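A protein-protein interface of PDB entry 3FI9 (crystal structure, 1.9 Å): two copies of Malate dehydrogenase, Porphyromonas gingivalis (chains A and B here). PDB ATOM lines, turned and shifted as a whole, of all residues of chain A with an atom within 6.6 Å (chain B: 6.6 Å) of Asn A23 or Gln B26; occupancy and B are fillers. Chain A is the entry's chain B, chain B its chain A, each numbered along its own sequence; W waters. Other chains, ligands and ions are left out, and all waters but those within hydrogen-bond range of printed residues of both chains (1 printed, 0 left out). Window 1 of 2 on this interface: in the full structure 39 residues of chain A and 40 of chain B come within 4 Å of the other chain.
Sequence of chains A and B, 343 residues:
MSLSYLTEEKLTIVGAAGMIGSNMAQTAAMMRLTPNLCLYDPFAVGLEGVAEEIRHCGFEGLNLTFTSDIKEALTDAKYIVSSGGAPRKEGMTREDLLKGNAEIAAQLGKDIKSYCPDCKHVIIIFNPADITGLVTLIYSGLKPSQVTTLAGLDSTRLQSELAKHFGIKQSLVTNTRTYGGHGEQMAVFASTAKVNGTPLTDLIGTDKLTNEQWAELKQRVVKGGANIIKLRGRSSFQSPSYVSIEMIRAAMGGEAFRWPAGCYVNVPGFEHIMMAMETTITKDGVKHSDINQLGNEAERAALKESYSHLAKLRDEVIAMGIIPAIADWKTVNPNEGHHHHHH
Ser A22 touches Gln B238, and with the chains exchanged Gln A238 touches Ser B22.
Asn A23 touches Gln B26, and with the chains exchanged Gln A26 touches Asn B23.
Gln A26 touches Thr B27, and with the chains exchanged Thr A27 touches Gln B26.
Met A30 touches its own counterpart, Met B30.
12 positions are printed for both chains.
The backbone carbonyl oxygen (O) of Asn B23 lies within hydrogen-bond range of the side-chain hydroxyl (OG1) of Thr B27 (2.9 Å).
NH1 of Arg B232 sits at hydrogen-bond distance from OE1 of Gln B238, 2.8 Å away.
O of Ala A16 sits at hydrogen-bond distance from N of Ser A22 (3.4 Å).
The side-chain hydroxyl (OG) of Ser A22 is in hydrogen-bond range of the backbone carbonyl oxygen (O) of Gly A18.
The side-chain hydroxyl (OG) of Ser A241 sits at hydrogen-bond distance from the side-chain amide oxygen (OD1) of Asn A23.
The side-chain amide nitrogen (NE2) of Gln A26 sits at hydrogen-bond distance from the side-chain sulfur (SD) of Met A30, 3.7 Å away.
Asn A23 touches just one residue of chain B: Gln B26.
Of the printed residues of chain B, Met A19 touches Phe B237.
Printed residues of chain A within 4 Å of Gln B238: Ser A22 (3.0 Å) and Gln A26 (2.9 Å).
Printed residues of chain B within 4 Å of Gln A26: Asn B23, Thr B27 and Gln B238.
Printed residues of chain A within 4 Å of Phe B59: Tyr A242.
Of the printed residues of chain A, Asn B23 touches Gln A26 (2.8 Å) and Gln A238 (3.996 Å).
Gly B21 touches none of the printed residues of chain A.
The nearest printed residue of chain B that does not touch Asn A23 is Gln B238 (4.03 Å).
The nearest residue of chain A that does not touch Gln B26 is Tyr A242 (4.1 Å).
The nearest printed residue of chain A that does not touch Phe B59 is Gln A238 (7.2 Å).
Of the 21 printed residues of chain A, 10 touch a printed residue of chain B.
Hydrophobic or aromatic side chains of chain B within 4 Å of the printed part of chain A: Met B30, Phe B59 and Phe B237.
Among the printed residues, no Asp or Glu carboxylate lies within 4 Å of a Lys or Arg side-chain nitrogen of the other chain.
The side-chain amide nitrogen (NE2) of Gln A238 is in hydrogen-bond range of the backbone carbonyl oxygen (O) of Ser B22, 3.1 Å away.
ND2 of Asn B23 lies within hydrogen-bond range of OE1 of Gln A26 (2.8 Å).
The side-chain amide oxygen (OE1) of Gln B26 lies within hydrogen-bond range of the side-chain amide nitrogen (ND2) of Asn A23.
NE2 of Gln B26 sits at hydrogen-bond distance from OG1 of Thr A27.
NE2 of Gln A238 is in hydrogen-bond range of OE1 of Gln B26, 2.9 Å away.
NE2 of Gln A26 sits at hydrogen-bond distance from OG1 of Thr B27.
NH2 of Arg B232 lies within hydrogen-bond range of OG of Ser A22 (3.0 Å).
NE2 of Gln B238 sits at hydrogen-bond distance from O of Ser A22.
The side-chain amide oxygen of Gln A26 lies within hydrogen-bond range of the side-chain amide nitrogen of Gln B238 (2.9 Å).
Water W1 lies within hydrogen-bond range of ND2 of Asn A23 and ND2 of Asn B23.
Among the printed residues, pairs that only touch across the chains: Tyr A242 with Phe B59 (3.4 Å), Tyr A242 with Cys B57 (3.6 Å), Thr A27 with Met B30 (3.6 Å), Ser A239 with Cys B57 (3.7 Å), Met A30 with Met B30 (3.8 Å), Tyr A242 with Met B30 (3.8 Å), Met A19 with Phe B237 (3.8 Å), Val A50 with Arg B232 (3.9 Å), Met A30 with Thr B27 (3.9 Å) and Gln A238 with Asn B23 (3.996 Å).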
ATOM      1  N   ALA A  16     -15.757  -8.765 -10.115  1.00  0.00           N
ATOM      2  CA  ALA A  16     -15.471 -10.174  -9.927  1.00  0.00           C
ATOM      3  C   ALA A  16     -16.691 -11.077 -10.194  1.00  0.00           C
ATOM      4  O   ALA A  16     -16.534 -12.277 -10.383  1.00  0.00           O
ATOM      5  CB  ALA A  16     -14.951 -10.393  -8.480  1.00  0.00           C
ATOM      6  N   GLY A  18     -18.722 -10.931 -12.778  1.00  0.00           N
ATOM      7  CA  GLY A  18     -18.798 -11.163 -14.204  1.00  0.00           C
ATOM      8  C   GLY A  18     -18.005 -12.332 -14.779  1.00  0.00           C
ATOM      9  O   GLY A  18     -17.253 -13.030 -14.074  1.00  0.00           O
ATOM     10  N   MET A  19     -18.211 -12.582 -16.078  1.00  0.00           N
ATOM     11  CA  MET A  19     -17.502 -13.688 -16.740  1.00  0.00           C
ATOM     12  C   MET A  19     -15.996 -13.442 -16.791  1.00  0.00           C
ATOM     13  O   MET A  19     -15.202 -14.368 -16.628  1.00  0.00           O
ATOM     14  CB  MET A  19     -18.062 -13.967 -18.137  1.00  0.00           C
ATOM     15  CG  MET A  19     -19.559 -14.449 -18.102  1.00  0.00           C
ATOM     16  SD  MET A  19     -19.779 -16.097 -17.416  1.00  0.00           S
ATOM     17  CE  MET A  19     -18.512 -16.940 -18.368  1.00  0.00           C
ATOM     18  N   ILE A  20     -15.593 -12.209 -17.042  1.00  0.00           N
ATOM     19  CA  ILE A  20     -14.171 -11.915 -17.042  1.00  0.00           C
ATOM     20  C   ILE A  20     -13.628 -11.983 -15.599  1.00  0.00           C
ATOM     21  O   ILE A  20     -12.572 -12.623 -15.333  1.00  0.00           O
ATOM     22  CB  ILE A  20     -13.846 -10.541 -17.637  1.00  0.00           C
ATOM     23  CG1 ILE A  20     -14.072 -10.513 -19.167  1.00  0.00           C
ATOM     24  CG2 ILE A  20     -12.402 -10.151 -17.358  1.00  0.00           C
ATOM     25  CD1 ILE A  20     -14.049  -9.103 -19.724  1.00  0.00           C
ATOM     26  N   GLY A  21     -14.302 -11.284 -14.689  1.00  0.00           N
ATOM     27  CA  GLY A  21     -13.804 -11.232 -13.305  1.00  0.00           C
ATOM     28  C   GLY A  21     -13.715 -12.607 -12.647  1.00  0.00           C
ATOM     29  O   GLY A  21     -12.801 -12.868 -11.855  1.00  0.00           O
ATOM     30  N   SER A  22     -14.671 -13.468 -12.933  1.00  0.00           N
ATOM     31  CA  SER A  22     -14.733 -14.762 -12.257  1.00  0.00           C
ATOM     32  C   SER A  22     -13.604 -15.643 -12.789  1.00  0.00           C
ATOM     33  O   SER A  22     -13.011 -16.426 -12.051  1.00  0.00           O
ATOM     34  CB  SER A  22     -16.114 -15.432 -12.431  1.00  0.00           C
ATOM     35  OG  SER A  22     -16.425 -15.709 -13.808  1.00  0.00           O
ATOM     36  N   ASN A  23     -13.314 -15.501 -14.086  1.00  0.00           N
ATOM     37  CA  ASN A  23     -12.217 -16.223 -14.688  1.00  0.00           C
ATOM     38  C   ASN A  23     -10.899 -15.669 -14.116  1.00  0.00           C
ATOM     39  O   ASN A  23      -9.971 -16.452 -13.844  1.00  0.00           O
ATOM     40  CB  ASN A  23     -12.241 -16.116 -16.210  1.00  0.00           C
ATOM     41  CG  ASN A  23     -11.194 -17.015 -16.875  1.00  0.00           C
ATOM     42  OD1 ASN A  23     -10.005 -16.696 -16.903  1.00  0.00           O
ATOM     43  ND2 ASN A  23     -11.639 -18.152 -17.402  1.00  0.00           N
ATOM     44  N   MET A  24     -10.836 -14.361 -13.893  1.00  0.00           N
ATOM     45  CA  MET A  24      -9.664 -13.749 -13.276  1.00  0.00           C
ATOM     46  C   MET A  24      -9.401 -14.325 -11.884  1.00  0.00           C
ATOM     47  O   MET A  24      -8.252 -14.538 -11.499  1.00  0.00           O
ATOM     48  CB  MET A  24      -9.834 -12.231 -13.194  1.00  0.00           C
ATOM     49  CG  MET A  24      -9.674 -11.514 -14.526  1.00  0.00           C
ATOM     50  SD  MET A  24      -9.295  -9.763 -14.333  1.00  0.00           S
ATOM     51  CE  MET A  24     -10.871  -9.136 -13.755  1.00  0.00           C
ATOM     52  N   ALA A  25     -10.472 -14.572 -11.134  1.00  0.00           N
ATOM     53  CA  ALA A  25     -10.362 -15.116  -9.778  1.00  0.00           C
ATOM     54  C   ALA A  25      -9.740 -16.498  -9.859  1.00  0.00           C
ATOM     55  O   ALA A  25      -8.825 -16.842  -9.100  1.00  0.00           O
ATOM     56  CB  ALA A  25     -11.780 -15.204  -9.131  1.00  0.00           C
ATOM     57  N   GLN A  26     -10.276 -17.339 -10.741  1.00  0.00           N
ATOM     58  CA  GLN A  26      -9.693 -18.665 -10.864  1.00  0.00           C
ATOM     59  C   GLN A  26      -8.221 -18.606 -11.321  1.00  0.00           C
ATOM     60  O   GLN A  26      -7.428 -19.381 -10.870  1.00  0.00           O
ATOM     61  CB  GLN A  26     -10.499 -19.515 -11.805  1.00  0.00           C
ATOM     62  CG  GLN A  26      -9.915 -20.913 -12.102  1.00  0.00           C
ATOM     63  CD  GLN A  26     -10.742 -21.628 -13.160  1.00  0.00           C
ATOM     64  OE1 GLN A  26     -11.874 -21.196 -13.507  1.00  0.00           O
ATOM     65  NE2 GLN A  26     -10.190 -22.718 -13.685  1.00  0.00           N
ATOM     66  N   THR A  27      -7.895 -17.731 -12.278  1.00  0.00           N
ATOM     67  CA  THR A  27      -6.535 -17.677 -12.822  1.00  0.00           C
ATOM     68  C   THR A  27      -5.544 -17.237 -11.746  1.00  0.00           C
ATOM     69  O   THR A  27      -4.425 -17.807 -11.626  1.00  0.00           O
ATOM     70  CB  THR A  27      -6.476 -16.733 -14.060  1.00  0.00           C
ATOM     71  OG1 THR A  27      -7.402 -17.236 -15.051  1.00  0.00           O
ATOM     72  CG2 THR A  27      -4.986 -16.664 -14.635  1.00  0.00           C
ATOM     73  N   ALA A  28      -5.934 -16.225 -10.982  1.00  0.00           N
ATOM     74  CA  ALA A  28      -5.074 -15.690  -9.903  1.00  0.00           C
ATOM     75  C   ALA A  28      -4.854 -16.744  -8.831  1.00  0.00           C
ATOM     76  O   ALA A  28      -3.744 -16.879  -8.305  1.00  0.00           O
ATOM     77  CB  ALA A  28      -5.711 -14.415  -9.278  1.00  0.00           C
ATOM     78  N   MET A  30      -5.056 -20.061  -9.338  1.00  0.00           N
ATOM     79  CA  MET A  30      -4.209 -21.093  -9.917  1.00  0.00           C
ATOM     80  C   MET A  30      -2.740 -20.694  -9.937  1.00  0.00           C
ATOM     81  O   MET A  30      -1.847 -21.539  -9.704  1.00  0.00           O
ATOM     82  CB  MET A  30      -4.653 -21.426 -11.359  1.00  0.00           C
ATOM     83  CG  MET A  30      -5.943 -22.272 -11.464  1.00  0.00           C
ATOM     84  SD  MET A  30      -6.519 -22.473 -13.221  1.00  0.00           S
ATOM     85  CE  MET A  30      -5.076 -23.480 -13.739  1.00  0.00           C
ATOM     86  N   VAL A  50     -19.859 -16.702  -7.523  1.00  0.00           N
ATOM     87  CA  VAL A  50     -18.459 -16.806  -8.005  1.00  0.00           C
ATOM     88  C   VAL A  50     -17.582 -17.261  -6.851  1.00  0.00           C
ATOM     89  O   VAL A  50     -16.829 -18.197  -7.025  1.00  0.00           O
ATOM     90  CB  VAL A  50     -17.945 -15.490  -8.602  1.00  0.00           C
ATOM     91  CG1 VAL A  50     -16.404 -15.561  -8.915  1.00  0.00           C
ATOM     92  CG2 VAL A  50     -18.759 -15.133  -9.872  1.00  0.00           C
ATOM     93  N   ILE A  54     -15.249 -20.684  -6.589  1.00  0.00           N
ATOM     94  CA  ILE A  54     -13.821 -20.686  -6.335  1.00  0.00           C
ATOM     95  C   ILE A  54     -13.522 -21.563  -5.100  1.00  0.00           C
ATOM     96  O   ILE A  54     -12.577 -22.341  -5.090  1.00  0.00           O
ATOM     97  CB  ILE A  54     -13.248 -19.258  -6.127  1.00  0.00           C
ATOM     98  CG1 ILE A  54     -13.510 -18.408  -7.369  1.00  0.00           C
ATOM     99  CG2 ILE A  54     -11.735 -19.294  -5.645  1.00  0.00           C
ATOM    100  CD1 ILE A  54     -12.836 -18.925  -8.661  1.00  0.00           C
ATOM    101  N   PHE A 237     -13.999 -13.426 -22.777  1.00  0.00           N
ATOM    102  CA  PHE A 237     -13.781 -13.309 -21.322  1.00  0.00           C
ATOM    103  C   PHE A 237     -12.579 -14.116 -20.836  1.00  0.00           C
ATOM    104  O   PHE A 237     -11.951 -13.756 -19.838  1.00  0.00           O
ATOM    105  CB  PHE A 237     -15.046 -13.660 -20.534  1.00  0.00           C
ATOM    106  CG  PHE A 237     -15.566 -15.061 -20.784  1.00  0.00           C
ATOM    107  CD1 PHE A 237     -15.368 -16.075 -19.854  1.00  0.00           C
ATOM    108  CD2 PHE A 237     -16.254 -15.354 -21.931  1.00  0.00           C
ATOM    109  CE1 PHE A 237     -15.867 -17.382 -20.103  1.00  0.00           C
ATOM    110  CE2 PHE A 237     -16.740 -16.656 -22.183  1.00  0.00           C
ATOM    111  CZ  PHE A 237     -16.551 -17.661 -21.272  1.00  0.00           C
ATOM    112  N   GLN A 238     -12.246 -15.196 -21.510  1.00  0.00           N
ATOM    113  CA  GLN A 238     -11.092 -15.986 -21.055  1.00  0.00           C
ATOM    114  C   GLN A 238      -9.742 -15.328 -21.365  1.00  0.00           C
ATOM    115  O   GLN A 238      -8.862 -15.239 -20.468  1.00  0.00           O
ATOM    116  CB  GLN A 238     -11.151 -17.387 -21.633  1.00  0.00           C
ATOM    117  CG  GLN A 238     -12.428 -18.096 -21.219  1.00  0.00           C
ATOM    118  CD  GLN A 238     -12.489 -19.532 -21.675  1.00  0.00           C
ATOM    119  OE1 GLN A 238     -13.316 -19.898 -22.517  1.00  0.00           O
ATOM    120  NE2 GLN A 238     -11.658 -20.371 -21.072  1.00  0.00           N
ATOM    121  N   SER A 239      -9.555 -14.894 -22.611  1.00  0.00           N
ATOM    122  CA  SER A 239      -8.293 -14.258 -22.978  1.00  0.00           C
ATOM    123  C   SER A 239      -7.994 -12.912 -22.256  1.00  0.00           C
ATOM    124  O   SER A 239      -6.891 -12.771 -21.745  1.00  0.00           O
ATOM    125  CB  SER A 239      -8.029 -14.216 -24.508  1.00  0.00           C
ATOM    126  OG  SER A 239      -9.064 -13.566 -25.228  1.00  0.00           O
ATOM    127  N   SER A 241      -9.060 -11.998 -19.443  1.00  0.00           N
ATOM    128  CA  SER A 241      -8.826 -12.379 -18.039  1.00  0.00           C
ATOM    129  C   SER A 241      -7.450 -12.950 -17.896  1.00  0.00           C
ATOM    130  O   SER A 241      -6.613 -12.468 -17.090  1.00  0.00           O
ATOM    131  CB  SER A 241      -9.875 -13.406 -17.574  1.00  0.00           C
ATOM    132  OG  SER A 241      -9.382 -14.060 -16.402  1.00  0.00           O
ATOM    133  N   TYR A 242      -7.153 -13.968 -18.695  1.00  0.00           N
ATOM    134  CA  TYR A 242      -5.849 -14.581 -18.611  1.00  0.00           C
ATOM    135  C   TYR A 242      -4.677 -13.572 -18.778  1.00  0.00           C
ATOM    136  O   TYR A 242      -3.723 -13.534 -17.944  1.00  0.00           O
ATOM    137  CB  TYR A 242      -5.680 -15.771 -19.600  1.00  0.00           C
ATOM    138  CG  TYR A 242      -4.311 -16.391 -19.492  1.00  0.00           C
ATOM    139  CD1 TYR A 242      -3.973 -17.216 -18.390  1.00  0.00           C
ATOM    140  CD2 TYR A 242      -3.332 -16.158 -20.456  1.00  0.00           C
ATOM    141  CE1 TYR A 242      -2.710 -17.776 -18.284  1.00  0.00           C
ATOM    142  CE2 TYR A 242      -2.036 -16.734 -20.339  1.00  0.00           C
ATOM    143  CZ  TYR A 242      -1.743 -17.526 -19.258  1.00  0.00           C
ATOM    144  OH  TYR A 242      -0.463 -18.062 -19.095  1.00  0.00           O
ATOM    145  N   ILE A 245      -4.216 -11.123 -15.838  1.00  0.00           N
ATOM    146  CA  ILE A 245      -3.678 -11.659 -14.584  1.00  0.00           C
ATOM    147  C   ILE A 245      -2.195 -12.018 -14.809  1.00  0.00           C
ATOM    148  O   ILE A 245      -1.365 -11.945 -13.876  1.00  0.00           O
ATOM    149  CB  ILE A 245      -4.547 -12.829 -14.105  1.00  0.00           C
ATOM    150  CG1 ILE A 245      -5.978 -12.315 -13.823  1.00  0.00           C
ATOM    151  CG2 ILE A 245      -3.956 -13.471 -12.875  1.00  0.00           C
ATOM    152  CD1 ILE A 245      -6.030 -11.095 -12.824  1.00  0.00           C
ATOM    153  N   GLY B  21     -16.333 -27.125 -20.709  1.00  0.00           N
ATOM    154  CA  GLY B  21     -15.228 -27.573 -21.606  1.00  0.00           C
ATOM    155  C   GLY B  21     -14.267 -26.445 -21.968  1.00  0.00           C
ATOM    156  O   GLY B  21     -13.052 -26.653 -22.099  1.00  0.00           O
ATOM    157  N   SER B  22     -14.794 -25.250 -22.179  1.00  0.00           N
ATOM    158  CA  SER B  22     -13.910 -24.121 -22.544  1.00  0.00           C
ATOM    159  C   SER B  22     -12.952 -23.784 -21.359  1.00  0.00           C
ATOM    160  O   SER B  22     -11.741 -23.463 -21.531  1.00  0.00           O
ATOM    161  CB  SER B  22     -14.728 -22.916 -23.033  1.00  0.00           C
ATOM    162  OG  SER B  22     -15.493 -22.273 -22.000  1.00  0.00           O
ATOM    163  N   ASN B  23     -13.503 -23.832 -20.153  1.00  0.00           N
ATOM    164  CA  ASN B  23     -12.704 -23.592 -18.951  1.00  0.00           C
ATOM    165  C   ASN B  23     -11.693 -24.705 -18.810  1.00  0.00           C
ATOM    166  O   ASN B  23     -10.571 -24.461 -18.428  1.00  0.00           O
ATOM    167  CB  ASN B  23     -13.594 -23.434 -17.710  1.00  0.00           C
ATOM    168  CG  ASN B  23     -12.796 -23.002 -16.455  1.00  0.00           C
ATOM    169  OD1 ASN B  23     -12.121 -23.806 -15.842  1.00  0.00           O
ATOM    170  ND2 ASN B  23     -12.937 -21.743 -16.057  1.00  0.00           N
ATOM    171  N   MET B  24     -12.060 -25.932 -19.184  1.00  0.00           N
ATOM    172  CA  MET B  24     -11.111 -27.039 -19.120  1.00  0.00           C
ATOM    173  C   MET B  24      -9.943 -26.803 -20.062  1.00  0.00           C
ATOM    174  O   MET B  24      -8.798 -27.105 -19.731  1.00  0.00           O
ATOM    175  CB  MET B  24     -11.773 -28.381 -19.478  1.00  0.00           C
ATOM    176  CG  MET B  24     -12.829 -28.927 -18.455  1.00  0.00           C
ATOM    177  SD  MET B  24     -13.558 -30.515 -19.211  1.00  0.00           S
ATOM    178  CE  MET B  24     -14.259 -31.234 -17.741  1.00  0.00           C
ATOM    179  N   ALA B  25     -10.245 -26.254 -21.220  1.00  0.00           N
ATOM    180  CA  ALA B  25      -9.209 -26.029 -22.198  1.00  0.00           C
ATOM    181  C   ALA B  25      -8.201 -25.039 -21.661  1.00  0.00           C
ATOM    182  O   ALA B  25      -7.006 -25.228 -21.818  1.00  0.00           O
ATOM    183  CB  ALA B  25      -9.823 -25.471 -23.531  1.00  0.00           C
ATOM    184  N   GLN B  26      -8.690 -23.963 -21.072  1.00  0.00           N
ATOM    185  CA  GLN B  26      -7.816 -22.931 -20.507  1.00  0.00           C
ATOM    186  C   GLN B  26      -7.032 -23.547 -19.336  1.00  0.00           C
ATOM    187  O   GLN B  26      -5.868 -23.294 -19.171  1.00  0.00           O
ATOM    188  CB  GLN B  26      -8.662 -21.721 -20.049  1.00  0.00           C
ATOM    189  CG  GLN B  26      -7.758 -20.632 -19.311  1.00  0.00           C
ATOM    190  CD  GLN B  26      -8.583 -19.478 -18.776  1.00  0.00           C
ATOM    191  OE1 GLN B  26      -9.753 -19.302 -19.132  1.00  0.00           O
ATOM    192  NE2 GLN B  26      -7.988 -18.705 -17.868  1.00  0.00           N
ATOM    193  N   THR B  27      -7.682 -24.384 -18.529  1.00  0.00           N
ATOM    194  CA  THR B  27      -6.996 -24.970 -17.388  1.00  0.00           C
ATOM    195  C   THR B  27      -5.902 -25.942 -17.808  1.00  0.00           C
ATOM    196  O   THR B  27      -4.786 -25.961 -17.224  1.00  0.00           O
ATOM    197  CB  THR B  27      -8.019 -25.641 -16.438  1.00  0.00           C
ATOM    198  OG1 THR B  27      -8.945 -24.635 -15.994  1.00  0.00           O
ATOM    199  CG2 THR B  27      -7.326 -26.295 -15.195  1.00  0.00           C
ATOM    200  N   ALA B  28      -6.211 -26.773 -18.788  1.00  0.00           N
ATOM    201  CA  ALA B  28      -5.218 -27.743 -19.266  1.00  0.00           C
ATOM    202  C   ALA B  28      -4.003 -27.028 -19.858  1.00  0.00           C
ATOM    203  O   ALA B  28      -2.849 -27.425 -19.629  1.00  0.00           O
ATOM    204  CB  ALA B  28      -5.847 -28.628 -20.342  1.00  0.00           C
ATOM    205  N   ALA B  29      -4.264 -25.972 -20.611  1.00  0.00           N
ATOM    206  CA  ALA B  29      -3.169 -25.176 -21.174  1.00  0.00           C
ATOM    207  C   ALA B  29      -2.350 -24.493 -20.087  1.00  0.00           C
ATOM    208  O   ALA B  29      -1.124 -24.514 -20.131  1.00  0.00           O
ATOM    209  CB  ALA B  29      -3.734 -24.145 -22.190  1.00  0.00           C
ATOM    210  N   MET B  30      -2.999 -23.871 -19.093  1.00  0.00           N
ATOM    211  CA  MET B  30      -2.218 -23.256 -18.022  1.00  0.00           C
ATOM    212  C   MET B  30      -1.340 -24.253 -17.298  1.00  0.00           C
ATOM    213  O   MET B  30      -0.212 -23.935 -16.878  1.00  0.00           O
ATOM    214  CB  MET B  30      -3.142 -22.585 -16.970  1.00  0.00           C
ATOM    215  CG  MET B  30      -3.832 -21.316 -17.465  1.00  0.00           C
ATOM    216  SD  MET B  30      -5.080 -20.555 -16.345  1.00  0.00           S
ATOM    217  CE  MET B  30      -3.889 -20.116 -14.990  1.00  0.00           C
ATOM    218  N   MET B  31      -1.888 -25.454 -17.075  1.00  0.00           N
ATOM    219  CA  MET B  31      -1.169 -26.482 -16.319  1.00  0.00           C
ATOM    220  C   MET B  31      -0.021 -27.110 -17.151  1.00  0.00           C
ATOM    221  O   MET B  31       0.704 -27.940 -16.655  1.00  0.00           O
ATOM    222  CB  MET B  31      -2.124 -27.596 -15.856  1.00  0.00           C
ATOM    223  CG  MET B  31      -3.003 -27.221 -14.634  1.00  0.00           C
ATOM    224  SD  MET B  31      -4.042 -28.680 -14.120  1.00  0.00           S
ATOM    225  CE  MET B  31      -4.963 -27.880 -12.791  1.00  0.00           C
ATOM    226  N   LEU B  37      -3.146 -30.346 -27.350  1.00  0.00           N
ATOM    227  CA  LEU B  37      -4.458 -30.256 -26.712  1.00  0.00           C
ATOM    228  C   LEU B  37      -5.490 -30.146 -27.813  1.00  0.00           C
ATOM    229  O   LEU B  37      -5.425 -29.254 -28.657  1.00  0.00           O
ATOM    230  CB  LEU B  37      -4.478 -29.008 -25.819  1.00  0.00           C
ATOM    231  CG  LEU B  37      -5.794 -28.716 -25.116  1.00  0.00           C
ATOM    232  CD1 LEU B  37      -6.020 -29.808 -24.129  1.00  0.00           C
ATOM    233  CD2 LEU B  37      -5.773 -27.292 -24.434  1.00  0.00           C
ATOM    234  N   ILE B  54      -8.622 -19.357 -26.758  1.00  0.00           N
ATOM    235  CA  ILE B  54      -7.426 -20.015 -26.235  1.00  0.00           C
ATOM    236  C   ILE B  54      -6.185 -19.536 -26.975  1.00  0.00           C
ATOM    237  O   ILE B  54      -5.170 -19.169 -26.369  1.00  0.00           O
ATOM    238  CB  ILE B  54      -7.541 -21.539 -26.326  1.00  0.00           C
ATOM    239  CG1 ILE B  54      -8.850 -21.971 -25.599  1.00  0.00           C
ATOM    240  CG2 ILE B  54      -6.223 -22.209 -25.852  1.00  0.00           C
ATOM    241  CD1 ILE B  54      -8.881 -21.561 -24.089  1.00  0.00           C
ATOM    242  N   CYS B  57      -4.819 -16.232 -25.795  1.00  0.00           N
ATOM    243  CA  CYS B  57      -4.127 -16.187 -24.487  1.00  0.00           C
ATOM    244  C   CYS B  57      -2.625 -16.193 -24.682  1.00  0.00           C
ATOM    245  O   CYS B  57      -1.867 -15.762 -23.795  1.00  0.00           O
ATOM    246  CB  CYS B  57      -4.485 -17.405 -23.646  1.00  0.00           C
ATOM    247  SG  CYS B  57      -6.173 -17.305 -23.041  1.00  0.00           S
ATOM    248  N   PHE B  59      -0.497 -19.088 -25.185  1.00  0.00           N
ATOM    249  CA  PHE B  59       0.185 -20.104 -24.409  1.00  0.00           C
ATOM    250  C   PHE B  59       1.415 -20.585 -25.154  1.00  0.00           C
ATOM    251  O   PHE B  59       1.285 -21.122 -26.261  1.00  0.00           O
ATOM    252  CB  PHE B  59      -0.740 -21.280 -24.128  1.00  0.00           C
ATOM    253  CG  PHE B  59      -1.842 -20.942 -23.157  1.00  0.00           C
ATOM    254  CD1 PHE B  59      -1.558 -20.722 -21.822  1.00  0.00           C
ATOM    255  CD2 PHE B  59      -3.175 -20.838 -23.600  1.00  0.00           C
ATOM    256  CE1 PHE B  59      -2.613 -20.414 -20.923  1.00  0.00           C
ATOM    257  CE2 PHE B  59      -4.205 -20.554 -22.710  1.00  0.00           C
ATOM    258  CZ  PHE B  59      -3.906 -20.327 -21.381  1.00  0.00           C
ATOM    259  N   ARG B 232     -25.449 -17.749  -9.535  1.00  0.00           N
ATOM    260  CA  ARG B 232     -24.802 -17.386 -10.786  1.00  0.00           C
ATOM    261  C   ARG B 232     -25.737 -17.277 -11.941  1.00  0.00           C
ATOM    262  O   ARG B 232     -25.357 -16.703 -12.938  1.00  0.00           O
ATOM    263  CB  ARG B 232     -23.725 -18.410 -11.214  1.00  0.00           C
ATOM    264  CG  ARG B 232     -22.519 -18.427 -10.339  1.00  0.00           C
ATOM    265  CD  ARG B 232     -21.372 -19.106 -11.106  1.00  0.00           C
ATOM    266  NE  ARG B 232     -20.782 -18.107 -11.997  1.00  0.00           N
ATOM    267  CZ  ARG B 232     -19.507 -18.148 -12.381  1.00  0.00           C
ATOM    268  NH1 ARG B 232     -18.765 -19.152 -11.939  1.00  0.00           N
ATOM    269  NH2 ARG B 232     -18.991 -17.198 -13.148  1.00  0.00           N
ATOM    270  N   PHE B 237     -19.475 -24.178 -13.506  1.00  0.00           N
ATOM    271  CA  PHE B 237     -18.632 -24.578 -14.640  1.00  0.00           C
ATOM    272  C   PHE B 237     -17.157 -24.450 -14.325  1.00  0.00           C
ATOM    273  O   PHE B 237     -16.307 -25.213 -14.857  1.00  0.00           O
ATOM    274  CB  PHE B 237     -19.020 -23.815 -15.907  1.00  0.00           C
ATOM    275  CG  PHE B 237     -18.900 -22.321 -15.779  1.00  0.00           C
ATOM    276  CD1 PHE B 237     -17.779 -21.668 -16.269  1.00  0.00           C
ATOM    277  CD2 PHE B 237     -19.914 -21.585 -15.208  1.00  0.00           C
ATOM    278  CE1 PHE B 237     -17.664 -20.267 -16.167  1.00  0.00           C
ATOM    279  CE2 PHE B 237     -19.807 -20.203 -15.097  1.00  0.00           C
ATOM    280  CZ  PHE B 237     -18.682 -19.545 -15.579  1.00  0.00           C
ATOM    281  N   GLN B 238     -16.822 -23.545 -13.422  1.00  0.00           N
ATOM    282  CA  GLN B 238     -15.414 -23.398 -13.116  1.00  0.00           C
ATOM    283  C   GLN B 238     -14.933 -24.505 -12.170  1.00  0.00           C
ATOM    284  O   GLN B 238     -13.833 -25.097 -12.392  1.00  0.00           O
ATOM    285  CB  GLN B 238     -15.117 -22.030 -12.540  1.00  0.00           C
ATOM    286  CG  GLN B 238     -15.431 -20.878 -13.488  1.00  0.00           C
ATOM    287  CD  GLN B 238     -15.116 -19.514 -12.826  1.00  0.00           C
ATOM    288  OE1 GLN B 238     -16.046 -18.725 -12.507  1.00  0.00           O
ATOM    289  NE2 GLN B 238     -13.812 -19.256 -12.566  1.00  0.00           N
HETATM  290  O   HOH W   1     -14.186 -19.446 -17.486  1.00  0.00           O
